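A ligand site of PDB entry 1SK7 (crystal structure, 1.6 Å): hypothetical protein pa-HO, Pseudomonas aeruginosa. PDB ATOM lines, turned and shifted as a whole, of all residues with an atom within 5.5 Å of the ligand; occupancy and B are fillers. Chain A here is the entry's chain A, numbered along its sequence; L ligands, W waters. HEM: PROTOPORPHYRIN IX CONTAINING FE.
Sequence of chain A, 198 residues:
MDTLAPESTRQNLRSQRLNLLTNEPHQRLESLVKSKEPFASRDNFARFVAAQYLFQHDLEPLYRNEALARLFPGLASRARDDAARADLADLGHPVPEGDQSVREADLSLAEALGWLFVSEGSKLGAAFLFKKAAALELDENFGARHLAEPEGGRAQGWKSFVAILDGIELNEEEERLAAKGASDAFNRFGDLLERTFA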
ATOM      1  N   ASN A  19      -5.845 -37.916  34.115  1.00  0.00           N
ATOM      2  CA  ASN A  19      -6.161 -37.962  32.699  1.00  0.00           C
ATOM      3  C   ASN A  19      -7.134 -39.118  32.432  1.00  0.00           C
ATOM      4  O   ASN A  19      -8.085 -38.974  31.670  1.00  0.00           O
ATOM      5  CB  ASN A  19      -4.872 -38.106  31.876  1.00  0.00           C
ATOM      6  CG  ASN A  19      -4.052 -36.826  31.860  1.00  0.00           C
ATOM      7  OD1 ASN A  19      -4.549 -35.739  32.204  1.00  0.00           O
ATOM      8  ND2 ASN A  19      -2.796 -36.928  31.417  1.00  0.00           N
ATOM      9  N   THR A  22     -10.624 -38.339  33.980  1.00  0.00           N
ATOM     10  CA  THR A  22     -11.404 -37.336  33.285  1.00  0.00           C
ATOM     11  C   THR A  22     -11.516 -37.524  31.785  1.00  0.00           C
ATOM     12  O   THR A  22     -12.036 -36.668  31.089  1.00  0.00           O
ATOM     13  CB  THR A  22     -10.847 -35.924  33.566  1.00  0.00           C
ATOM     14  OG1 THR A  22      -9.543 -35.827  32.990  1.00  0.00           O
ATOM     15  CG2 THR A  22     -10.780 -35.656  35.079  1.00  0.00           C
ATOM     16  N   HIS A  26     -14.232 -35.446  29.593  1.00  0.00           N
ATOM     17  CA  HIS A  26     -13.702 -34.613  28.521  1.00  0.00           C
ATOM     18  C   HIS A  26     -14.381 -34.873  27.196  1.00  0.00           C
ATOM     19  O   HIS A  26     -14.734 -33.944  26.470  1.00  0.00           O
ATOM     20  CB  HIS A  26     -12.196 -34.815  28.379  1.00  0.00           C
ATOM     21  CG  HIS A  26     -11.573 -33.854  27.444  1.00  0.00           C
ATOM     22  ND1 HIS A  26     -11.699 -33.949  26.077  1.00  0.00           N
ATOM     23  CD2 HIS A  26     -10.945 -32.681  27.673  1.00  0.00           C
ATOM     24  CE1 HIS A  26     -11.180 -32.889  25.507  1.00  0.00           C
ATOM     25  NE2 HIS A  26     -10.715 -32.103  26.462  1.00  0.00           N
ATOM     26  N   LEU A  29     -17.746 -33.370  27.370  1.00  0.00           N
ATOM     27  CA  LEU A  29     -17.678 -31.912  27.298  1.00  0.00           C
ATOM     28  C   LEU A  29     -17.337 -31.475  25.885  1.00  0.00           C
ATOM     29  O   LEU A  29     -17.929 -30.531  25.364  1.00  0.00           O
ATOM     30  CB  LEU A  29     -16.638 -31.376  28.294  1.00  0.00           C
ATOM     31  CG  LEU A  29     -16.718 -29.878  28.562  1.00  0.00           C
ATOM     32  CD1 LEU A  29     -15.860 -29.523  29.760  1.00  0.00           C
ATOM     33  CD2 LEU A  29     -16.267 -29.115  27.359  1.00  0.00           C
ATOM     34  N   GLU A  30     -16.395 -32.142  25.235  1.00  0.00           N
ATOM     35  CA  GLU A  30     -16.076 -31.743  23.877  1.00  0.00           C
ATOM     36  C   GLU A  30     -17.310 -31.885  22.991  1.00  0.00           C
ATOM     37  O   GLU A  30     -17.569 -31.040  22.144  1.00  0.00           O
ATOM     38  CB  GLU A  30     -14.919 -32.565  23.300  1.00  0.00           C
ATOM     39  CG  GLU A  30     -14.275 -31.830  22.135  1.00  0.00           C
ATOM     40  CD  GLU A  30     -13.163 -32.585  21.457  1.00  0.00           C
ATOM     41  OE1 GLU A  30     -12.373 -33.275  22.152  1.00  0.00           O
ATOM     42  OE2 GLU A  30     -13.052 -32.467  20.220  1.00  0.00           O
ATOM     43  N   VAL A  33     -19.745 -28.972  23.669  1.00  0.00           N
ATOM     44  CA  VAL A  33     -19.322 -27.732  23.005  1.00  0.00           C
ATOM     45  C   VAL A  33     -19.655 -27.786  21.508  1.00  0.00           C
ATOM     46  O   VAL A  33     -20.253 -26.865  20.969  1.00  0.00           O
ATOM     47  CB  VAL A  33     -17.822 -27.472  23.203  1.00  0.00           C
ATOM     48  CG1 VAL A  33     -17.351 -26.306  22.306  1.00  0.00           C
ATOM     49  CG2 VAL A  33     -17.589 -27.128  24.650  1.00  0.00           C
ATOM     50  N   GLN A  52     -16.739 -19.275  29.482  1.00  0.00           N
ATOM     51  CA  GLN A  52     -15.318 -19.215  29.888  1.00  0.00           C
ATOM     52  C   GLN A  52     -15.135 -18.151  30.947  1.00  0.00           C
ATOM     53  O   GLN A  52     -14.435 -18.333  31.952  1.00  0.00           O
ATOM     54  CB  GLN A  52     -14.467 -18.882  28.682  1.00  0.00           C
ATOM     55  CG  GLN A  52     -14.515 -19.937  27.600  1.00  0.00           C
ATOM     56  CD  GLN A  52     -13.293 -20.827  27.572  1.00  0.00           C
ATOM     57  OE1 GLN A  52     -12.983 -21.516  28.551  1.00  0.00           O
ATOM     58  NE2 GLN A  52     -12.579 -20.813  26.448  1.00  0.00           N
ATOM     59  N   PHE A  55     -16.391 -19.338  34.250  1.00  0.00           N
ATOM     60  CA  PHE A  55     -15.494 -20.347  34.833  1.00  0.00           C
ATOM     61  C   PHE A  55     -14.316 -19.608  35.485  1.00  0.00           C
ATOM     62  O   PHE A  55     -13.845 -20.003  36.551  1.00  0.00           O
ATOM     63  CB  PHE A  55     -15.025 -21.305  33.724  1.00  0.00           C
ATOM     64  CG  PHE A  55     -14.380 -22.579  34.229  1.00  0.00           C
ATOM     65  CD1 PHE A  55     -15.038 -23.424  35.114  1.00  0.00           C
ATOM     66  CD2 PHE A  55     -13.137 -22.958  33.728  1.00  0.00           C
ATOM     67  CE1 PHE A  55     -14.470 -24.655  35.511  1.00  0.00           C
ATOM     68  CE2 PHE A  55     -12.563 -24.177  34.123  1.00  0.00           C
ATOM     69  CZ  PHE A  55     -13.238 -25.014  35.003  1.00  0.00           C
ATOM     70  N   PHE A 117      -6.060 -28.206  37.742  1.00  0.00           N
ATOM     71  CA  PHE A 117      -5.691 -29.145  36.707  1.00  0.00           C
ATOM     72  C   PHE A 117      -6.629 -28.969  35.511  1.00  0.00           C
ATOM     73  O   PHE A 117      -6.193 -28.906  34.367  1.00  0.00           O
ATOM     74  CB  PHE A 117      -5.704 -30.572  37.242  1.00  0.00           C
ATOM     75  CG  PHE A 117      -5.800 -31.625  36.174  1.00  0.00           C
ATOM     76  CD1 PHE A 117      -4.669 -32.062  35.519  1.00  0.00           C
ATOM     77  CD2 PHE A 117      -7.038 -32.173  35.840  1.00  0.00           C
ATOM     78  CE1 PHE A 117      -4.759 -33.030  34.537  1.00  0.00           C
ATOM     79  CE2 PHE A 117      -7.128 -33.141  34.859  1.00  0.00           C
ATOM     80  CZ  PHE A 117      -5.981 -33.569  34.205  1.00  0.00           C
ATOM     81  N   VAL A 118      -7.941 -28.894  35.811  1.00  0.00           N
ATOM     82  CA  VAL A 118      -8.910 -28.778  34.716  1.00  0.00           C
ATOM     83  C   VAL A 118      -8.819 -27.391  34.027  1.00  0.00           C
ATOM     84  O   VAL A 118      -8.842 -27.307  32.810  1.00  0.00           O
ATOM     85  CB  VAL A 118     -10.359 -29.049  35.228  1.00  0.00           C
ATOM     86  CG1 VAL A 118     -11.373 -28.845  34.072  1.00  0.00           C
ATOM     87  CG2 VAL A 118     -10.439 -30.508  35.744  1.00  0.00           C
ATOM     88  N   GLY A 121      -5.679 -27.354  31.973  1.00  0.00           N
ATOM     89  CA  GLY A 121      -5.793 -28.262  30.844  1.00  0.00           C
ATOM     90  C   GLY A 121      -6.726 -27.741  29.772  1.00  0.00           C
ATOM     91  O   GLY A 121      -6.557 -28.050  28.590  1.00  0.00           O
ATOM     92  N   SER A 122      -7.720 -26.956  30.179  1.00  0.00           N
ATOM     93  CA  SER A 122      -8.671 -26.414  29.216  1.00  0.00           C
ATOM     94  C   SER A 122      -7.995 -25.480  28.201  1.00  0.00           C
ATOM     95  O   SER A 122      -8.592 -25.137  27.175  1.00  0.00           O
ATOM     96  CB  SER A 122      -9.787 -25.682  29.956  1.00  0.00           C
ATOM     97  OG  SER A 122      -9.327 -24.437  30.442  1.00  0.00           O
ATOM     98  N   LEU A 124      -5.293 -26.275  26.555  1.00  0.00           N
ATOM     99  CA  LEU A 124      -4.716 -27.090  25.508  1.00  0.00           C
ATOM    100  C   LEU A 124      -5.594 -27.108  24.257  1.00  0.00           C
ATOM    101  O   LEU A 124      -6.831 -27.238  24.332  1.00  0.00           O
ATOM    102  CB  LEU A 124      -4.480 -28.508  26.017  1.00  0.00           C
ATOM    103  CG  LEU A 124      -3.424 -28.579  27.125  1.00  0.00           C
ATOM    104  CD1 LEU A 124      -3.454 -29.952  27.778  1.00  0.00           C
ATOM    105  CD2 LEU A 124      -2.061 -28.290  26.537  1.00  0.00           C
ATOM    106  N   GLY A 125      -4.951 -26.966  23.111  1.00  0.00           N
ATOM    107  CA  GLY A 125      -5.650 -26.971  21.850  1.00  0.00           C
ATOM    108  C   GLY A 125      -6.356 -25.660  21.562  1.00  0.00           C
ATOM    109  O   GLY A 125      -6.998 -25.517  20.523  1.00  0.00           O
ATOM    110  N   PHE A 128      -6.513 -24.137  18.237  1.00  0.00           N
ATOM    111  CA  PHE A 128      -7.484 -24.633  17.267  1.00  0.00           C
ATOM    112  C   PHE A 128      -8.747 -23.793  17.319  1.00  0.00           C
ATOM    113  O   PHE A 128      -9.356 -23.499  16.293  1.00  0.00           O
ATOM    114  CB  PHE A 128      -7.812 -26.112  17.562  1.00  0.00           C
ATOM    115  CG  PHE A 128      -6.673 -27.051  17.283  1.00  0.00           C
ATOM    116  CD1 PHE A 128      -6.706 -28.354  17.768  1.00  0.00           C
ATOM    117  CD2 PHE A 128      -5.567 -26.642  16.548  1.00  0.00           C
ATOM    118  CE1 PHE A 128      -5.646 -29.249  17.525  1.00  0.00           C
ATOM    119  CE2 PHE A 128      -4.499 -27.527  16.290  1.00  0.00           C
ATOM    120  CZ  PHE A 128      -4.543 -28.823  16.787  1.00  0.00           C
ATOM    121  N   LEU A 129      -9.143 -23.415  18.537  1.00  0.00           N
ATOM    122  CA  LEU A 129     -10.312 -22.580  18.745  1.00  0.00           C
ATOM    123  C   LEU A 129      -9.962 -21.200  18.224  1.00  0.00           C
ATOM    124  O   LEU A 129     -10.792 -20.520  17.620  1.00  0.00           O
ATOM    125  CB  LEU A 129     -10.663 -22.488  20.237  1.00  0.00           C
ATOM    126  CG  LEU A 129     -11.123 -23.741  20.978  1.00  0.00           C
ATOM    127  CD1 LEU A 129     -11.407 -23.384  22.431  1.00  0.00           C
ATOM    128  CD2 LEU A 129     -12.357 -24.319  20.308  1.00  0.00           C
ATOM    129  N   LYS A 132     -10.288 -21.277  14.529  1.00  0.00           N
ATOM    130  CA  LYS A 132     -11.679 -21.306  14.107  1.00  0.00           C
ATOM    131  C   LYS A 132     -12.343 -19.943  14.326  1.00  0.00           C
ATOM    132  O   LYS A 132     -13.255 -19.563  13.583  1.00  0.00           O
ATOM    133  CB  LYS A 132     -12.461 -22.408  14.831  1.00  0.00           C
ATOM    134  CG  LYS A 132     -12.062 -23.821  14.403  1.00  0.00           C
ATOM    135  CD  LYS A 132     -12.898 -24.874  15.116  1.00  0.00           C
ATOM    136  CE  LYS A 132     -12.407 -26.285  14.820  1.00  0.00           C
ATOM    137  NZ  LYS A 132     -12.905 -27.262  15.815  1.00  0.00           N
ATOM    138  N   ARG A 154       1.738 -22.691  24.712  1.00  0.00           N
ATOM    139  CA  ARG A 154       0.813 -23.573  25.421  1.00  0.00           C
ATOM    140  C   ARG A 154       1.490 -24.815  25.991  1.00  0.00           C
ATOM    141  O   ARG A 154       1.295 -25.178  27.152  1.00  0.00           O
ATOM    142  CB  ARG A 154      -0.307 -24.031  24.484  1.00  0.00           C
ATOM    143  CG  ARG A 154      -1.015 -22.937  23.719  1.00  0.00           C
ATOM    144  CD  ARG A 154      -2.027 -23.577  22.777  1.00  0.00           C
ATOM    145  NE  ARG A 154      -1.372 -24.533  21.880  1.00  0.00           N
ATOM    146  CZ  ARG A 154      -1.999 -25.324  21.016  1.00  0.00           C
ATOM    147  NH1 ARG A 154      -3.324 -25.278  20.919  1.00  0.00           N
ATOM    148  NH2 ARG A 154      -1.302 -26.144  20.246  1.00  0.00           N
ATOM    149  N   TRP A 158       1.874 -26.036  30.134  1.00  0.00           N
ATOM    150  CA  TRP A 158       1.254 -27.221  30.697  1.00  0.00           C
ATOM    151  C   TRP A 158       2.279 -28.139  31.386  1.00  0.00           C
ATOM    152  O   TRP A 158       2.051 -28.628  32.486  1.00  0.00           O
ATOM    153  CB  TRP A 158       0.503 -27.991  29.604  1.00  0.00           C
ATOM    154  CG  TRP A 158      -0.058 -29.306  30.049  1.00  0.00           C
ATOM    155  CD1 TRP A 158       0.357 -30.548  29.649  1.00  0.00           C
ATOM    156  CD2 TRP A 158      -1.101 -29.517  30.989  1.00  0.00           C
ATOM    157  NE1 TRP A 158      -0.376 -31.518  30.290  1.00  0.00           N
ATOM    158  CE2 TRP A 158      -1.280 -30.914  31.118  1.00  0.00           C
ATOM    159  CE3 TRP A 158      -1.916 -28.662  31.754  1.00  0.00           C
ATOM    160  CZ2 TRP A 158      -2.236 -31.471  31.971  1.00  0.00           C
ATOM    161  CZ3 TRP A 158      -2.862 -29.226  32.596  1.00  0.00           C
ATOM    162  CH2 TRP A 158      -3.015 -30.607  32.697  1.00  0.00           C
ATOM    163  N   ALA A 185     -15.089 -29.858  38.444  1.00  0.00           N
ATOM    164  CA  ALA A 185     -14.821 -28.761  37.504  1.00  0.00           C
ATOM    165  C   ALA A 185     -15.329 -29.045  36.088  1.00  0.00           C
ATOM    166  O   ALA A 185     -15.840 -28.158  35.417  1.00  0.00           O
ATOM    167  CB  ALA A 185     -13.316 -28.417  37.483  1.00  0.00           C
ATOM    168  N   PHE A 186     -15.189 -30.286  35.613  1.00  0.00           N
ATOM    169  CA  PHE A 186     -15.717 -30.612  34.290  1.00  0.00           C
ATOM    170  C   PHE A 186     -17.249 -30.460  34.306  1.00  0.00           C
ATOM    171  O   PHE A 186     -17.827 -29.887  33.363  1.00  0.00           O
ATOM    172  CB  PHE A 186     -15.368 -32.059  33.904  1.00  0.00           C
ATOM    173  CG  PHE A 186     -14.134 -32.176  33.080  1.00  0.00           C
ATOM    174  CD1 PHE A 186     -12.916 -32.518  33.676  1.00  0.00           C
ATOM    175  CD2 PHE A 186     -14.157 -31.900  31.725  1.00  0.00           C
ATOM    176  CE1 PHE A 186     -11.752 -32.567  32.938  1.00  0.00           C
ATOM    177  CE2 PHE A 186     -12.984 -31.950  30.951  1.00  0.00           C
ATOM    178  CZ  PHE A 186     -11.766 -32.282  31.567  1.00  0.00           C
ATOM    179  N   PHE A 189     -18.214 -26.706  34.197  1.00  0.00           N
ATOM    180  CA  PHE A 189     -18.115 -26.040  32.904  1.00  0.00           C
ATOM    181  C   PHE A 189     -19.331 -26.408  32.065  1.00  0.00           C
ATOM    182  O   PHE A 189     -19.892 -25.571  31.359  1.00  0.00           O
ATOM    183  CB  PHE A 189     -16.824 -26.409  32.145  1.00  0.00           C
ATOM    184  CG  PHE A 189     -16.502 -25.437  31.034  1.00  0.00           C
ATOM    185  CD1 PHE A 189     -15.784 -24.287  31.312  1.00  0.00           C
ATOM    186  CD2 PHE A 189     -16.966 -25.633  29.740  1.00  0.00           C
ATOM    187  CE1 PHE A 189     -15.539 -23.320  30.313  1.00  0.00           C
ATOM    188  CE2 PHE A 189     -16.734 -24.678  28.727  1.00  0.00           C
ATOM    189  CZ  PHE A 189     -16.017 -23.518  29.024  1.00  0.00           C
HETATM  190  CHA HEM L   1      -9.202 -30.416  23.025  1.00  0.00           C
HETATM  191  CHB HEM L   1     -12.553 -28.315  25.750  1.00  0.00           C
HETATM  192  CHC HEM L   1     -10.188 -29.595  29.795  1.00  0.00           C
HETATM  193  CHD HEM L   1      -6.764 -31.609  27.037  1.00  0.00           C
HETATM  194  C1A HEM L   1     -10.379 -29.824  23.439  1.00  0.00           C
HETATM  195  C2A HEM L   1     -11.377 -29.253  22.536  1.00  0.00           C
HETATM  196  C3A HEM L   1     -12.343 -28.686  23.317  1.00  0.00           C
HETATM  197  C4A HEM L   1     -11.880 -28.824  24.668  1.00  0.00           C
HETATM  198  CMA HEM L   1     -13.728 -28.170  22.900  1.00  0.00           C
HETATM  199  CAA HEM L   1     -11.407 -29.287  20.998  1.00  0.00           C
HETATM  200  CBA HEM L   1     -10.633 -28.111  20.397  1.00  0.00           C
HETATM  201  CGA HEM L   1     -10.795 -28.021  18.894  1.00  0.00           C
HETATM  202  O1A HEM L   1     -11.855 -27.537  18.428  1.00  0.00           O
HETATM  203  O2A HEM L   1      -9.859 -28.447  18.175  1.00  0.00           O
HETATM  204  C1B HEM L   1     -12.165 -28.448  27.087  1.00  0.00           C
HETATM  205  C2B HEM L   1     -12.890 -27.862  28.204  1.00  0.00           C
HETATM  206  C3B HEM L   1     -12.274 -28.298  29.338  1.00  0.00           C
HETATM  207  C4B HEM L   1     -11.125 -29.060  28.902  1.00  0.00           C
HETATM  208  CMB HEM L   1     -14.057 -26.803  28.150  1.00  0.00           C
HETATM  209  CAB HEM L   1     -12.694 -28.111  30.655  1.00  0.00           C
HETATM  210  CBB HEM L   1     -13.404 -27.055  31.203  1.00  0.00           C
HETATM  211  C1C HEM L   1      -9.066 -30.324  29.392  1.00  0.00           C
HETATM  212  C2C HEM L   1      -8.117 -30.975  30.295  1.00  0.00           C
HETATM  213  C3C HEM L   1      -7.195 -31.535  29.519  1.00  0.00           C
HETATM  214  C4C HEM L   1      -7.536 -31.231  28.135  1.00  0.00           C
HETATM  215  CMC HEM L   1      -8.137 -31.003  31.829  1.00  0.00           C
HETATM  216  CAC HEM L   1      -5.993 -32.199  29.854  1.00  0.00           C
HETATM  217  CBC HEM L   1      -5.604 -32.658  31.123  1.00  0.00           C
HETATM  218  C1D HEM L   1      -7.117 -31.397  25.705  1.00  0.00           C
HETATM  219  C2D HEM L   1      -6.249 -31.740  24.565  1.00  0.00           C
HETATM  220  C3D HEM L   1      -6.979 -31.454  23.426  1.00  0.00           C
HETATM  221  C4D HEM L   1      -8.228 -30.893  23.884  1.00  0.00           C
HETATM  222  CMD HEM L   1      -4.880 -32.424  24.610  1.00  0.00           C
HETATM  223  CAD HEM L   1      -6.597 -31.796  21.972  1.00  0.00           C
HETATM  224  CBD HEM L   1      -5.436 -30.874  21.608  1.00  0.00           C
HETATM  225  CGD HEM L   1      -4.799 -31.210  20.275  1.00  0.00           C
HETATM  226  O1D HEM L   1      -3.636 -30.790  20.045  1.00  0.00           O
HETATM  227  O2D HEM L   1      -5.452 -31.873  19.441  1.00  0.00           O
HETATM  228  NA  HEM L   1     -10.698 -29.555  24.735  1.00  0.00           N
HETATM  229  NB  HEM L   1     -11.047 -29.173  27.507  1.00  0.00           N
HETATM  230  NC  HEM L   1      -8.722 -30.515  28.056  1.00  0.00           N
HETATM  231  ND  HEM L   1      -8.307 -30.851  25.286  1.00  0.00           N
HETATM  232 FE   HEM L   1      -9.677 -30.024  26.395  1.00  0.00          FE
HETATM  233  O   HOH W   1      -8.687 -28.378  26.213  1.00  0.00           O
HETATM  234  O   HOH W   2      -2.335 -33.517  20.332  1.00  0.00           O
HETATM  235  O   HOH W   3     -15.886 -29.630  20.635  1.00  0.00           O
HETATM  236  O   HOH W   4     -12.436 -24.310  27.626  1.00  0.00           O
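A ring nitrogen (NE2) of His 26 is bound to an iron atom (FE) of the ligand.
NZ of Lys 132 lies within salt-bridge range of O1A of the ligand.
NC of the ligand sits close to O of Gly 121.
Asn 19 touches the ligand.
Leu 29 touches the ligand.
Glu 30 touches the ligand.
Phe 117 touches the ligand.
CA of Val 118 touches CMC of the ligand, at 3.7 Å.
Ser 122 touches the ligand.
Leu 124 touches the ligand (CD1 to CHD, 3.8 Å).
Gly 125 touches the ligand (CA to CBD, 3.9 Å).
Phe 128 touches the ligand (CB to O2A, 3.2 Å).
Leu 129 touches the ligand (CD2 to O1A, 3.8 Å).
Trp 158 touches the ligand.
Phe 186 touches the ligand.
Phe 189 touches the ligand.
Hydrophobic or aromatic side chains within 4 Å of the ligand: His 26, Leu 29, Phe 117, Val 118, Leu 124, Phe 128, Leu 129, Trp 158, Phe 186 and Phe 189.
16 residues have an atom within 4 Å of the ligand: Asn 19, His 26, Leu 29, Glu 30, Phe 117, Val 118, Gly 121, Ser 122, Leu 124, Gly 125, Phe 128, Leu 129, Lys 132, Trp 158, Phe 186 and Phe 189.
Along chain A the residues within 4 Å of the ligand span positions 19 to 189.
The nearest printed residue that does not touch the ligand is Val 33 (4.1 Å).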
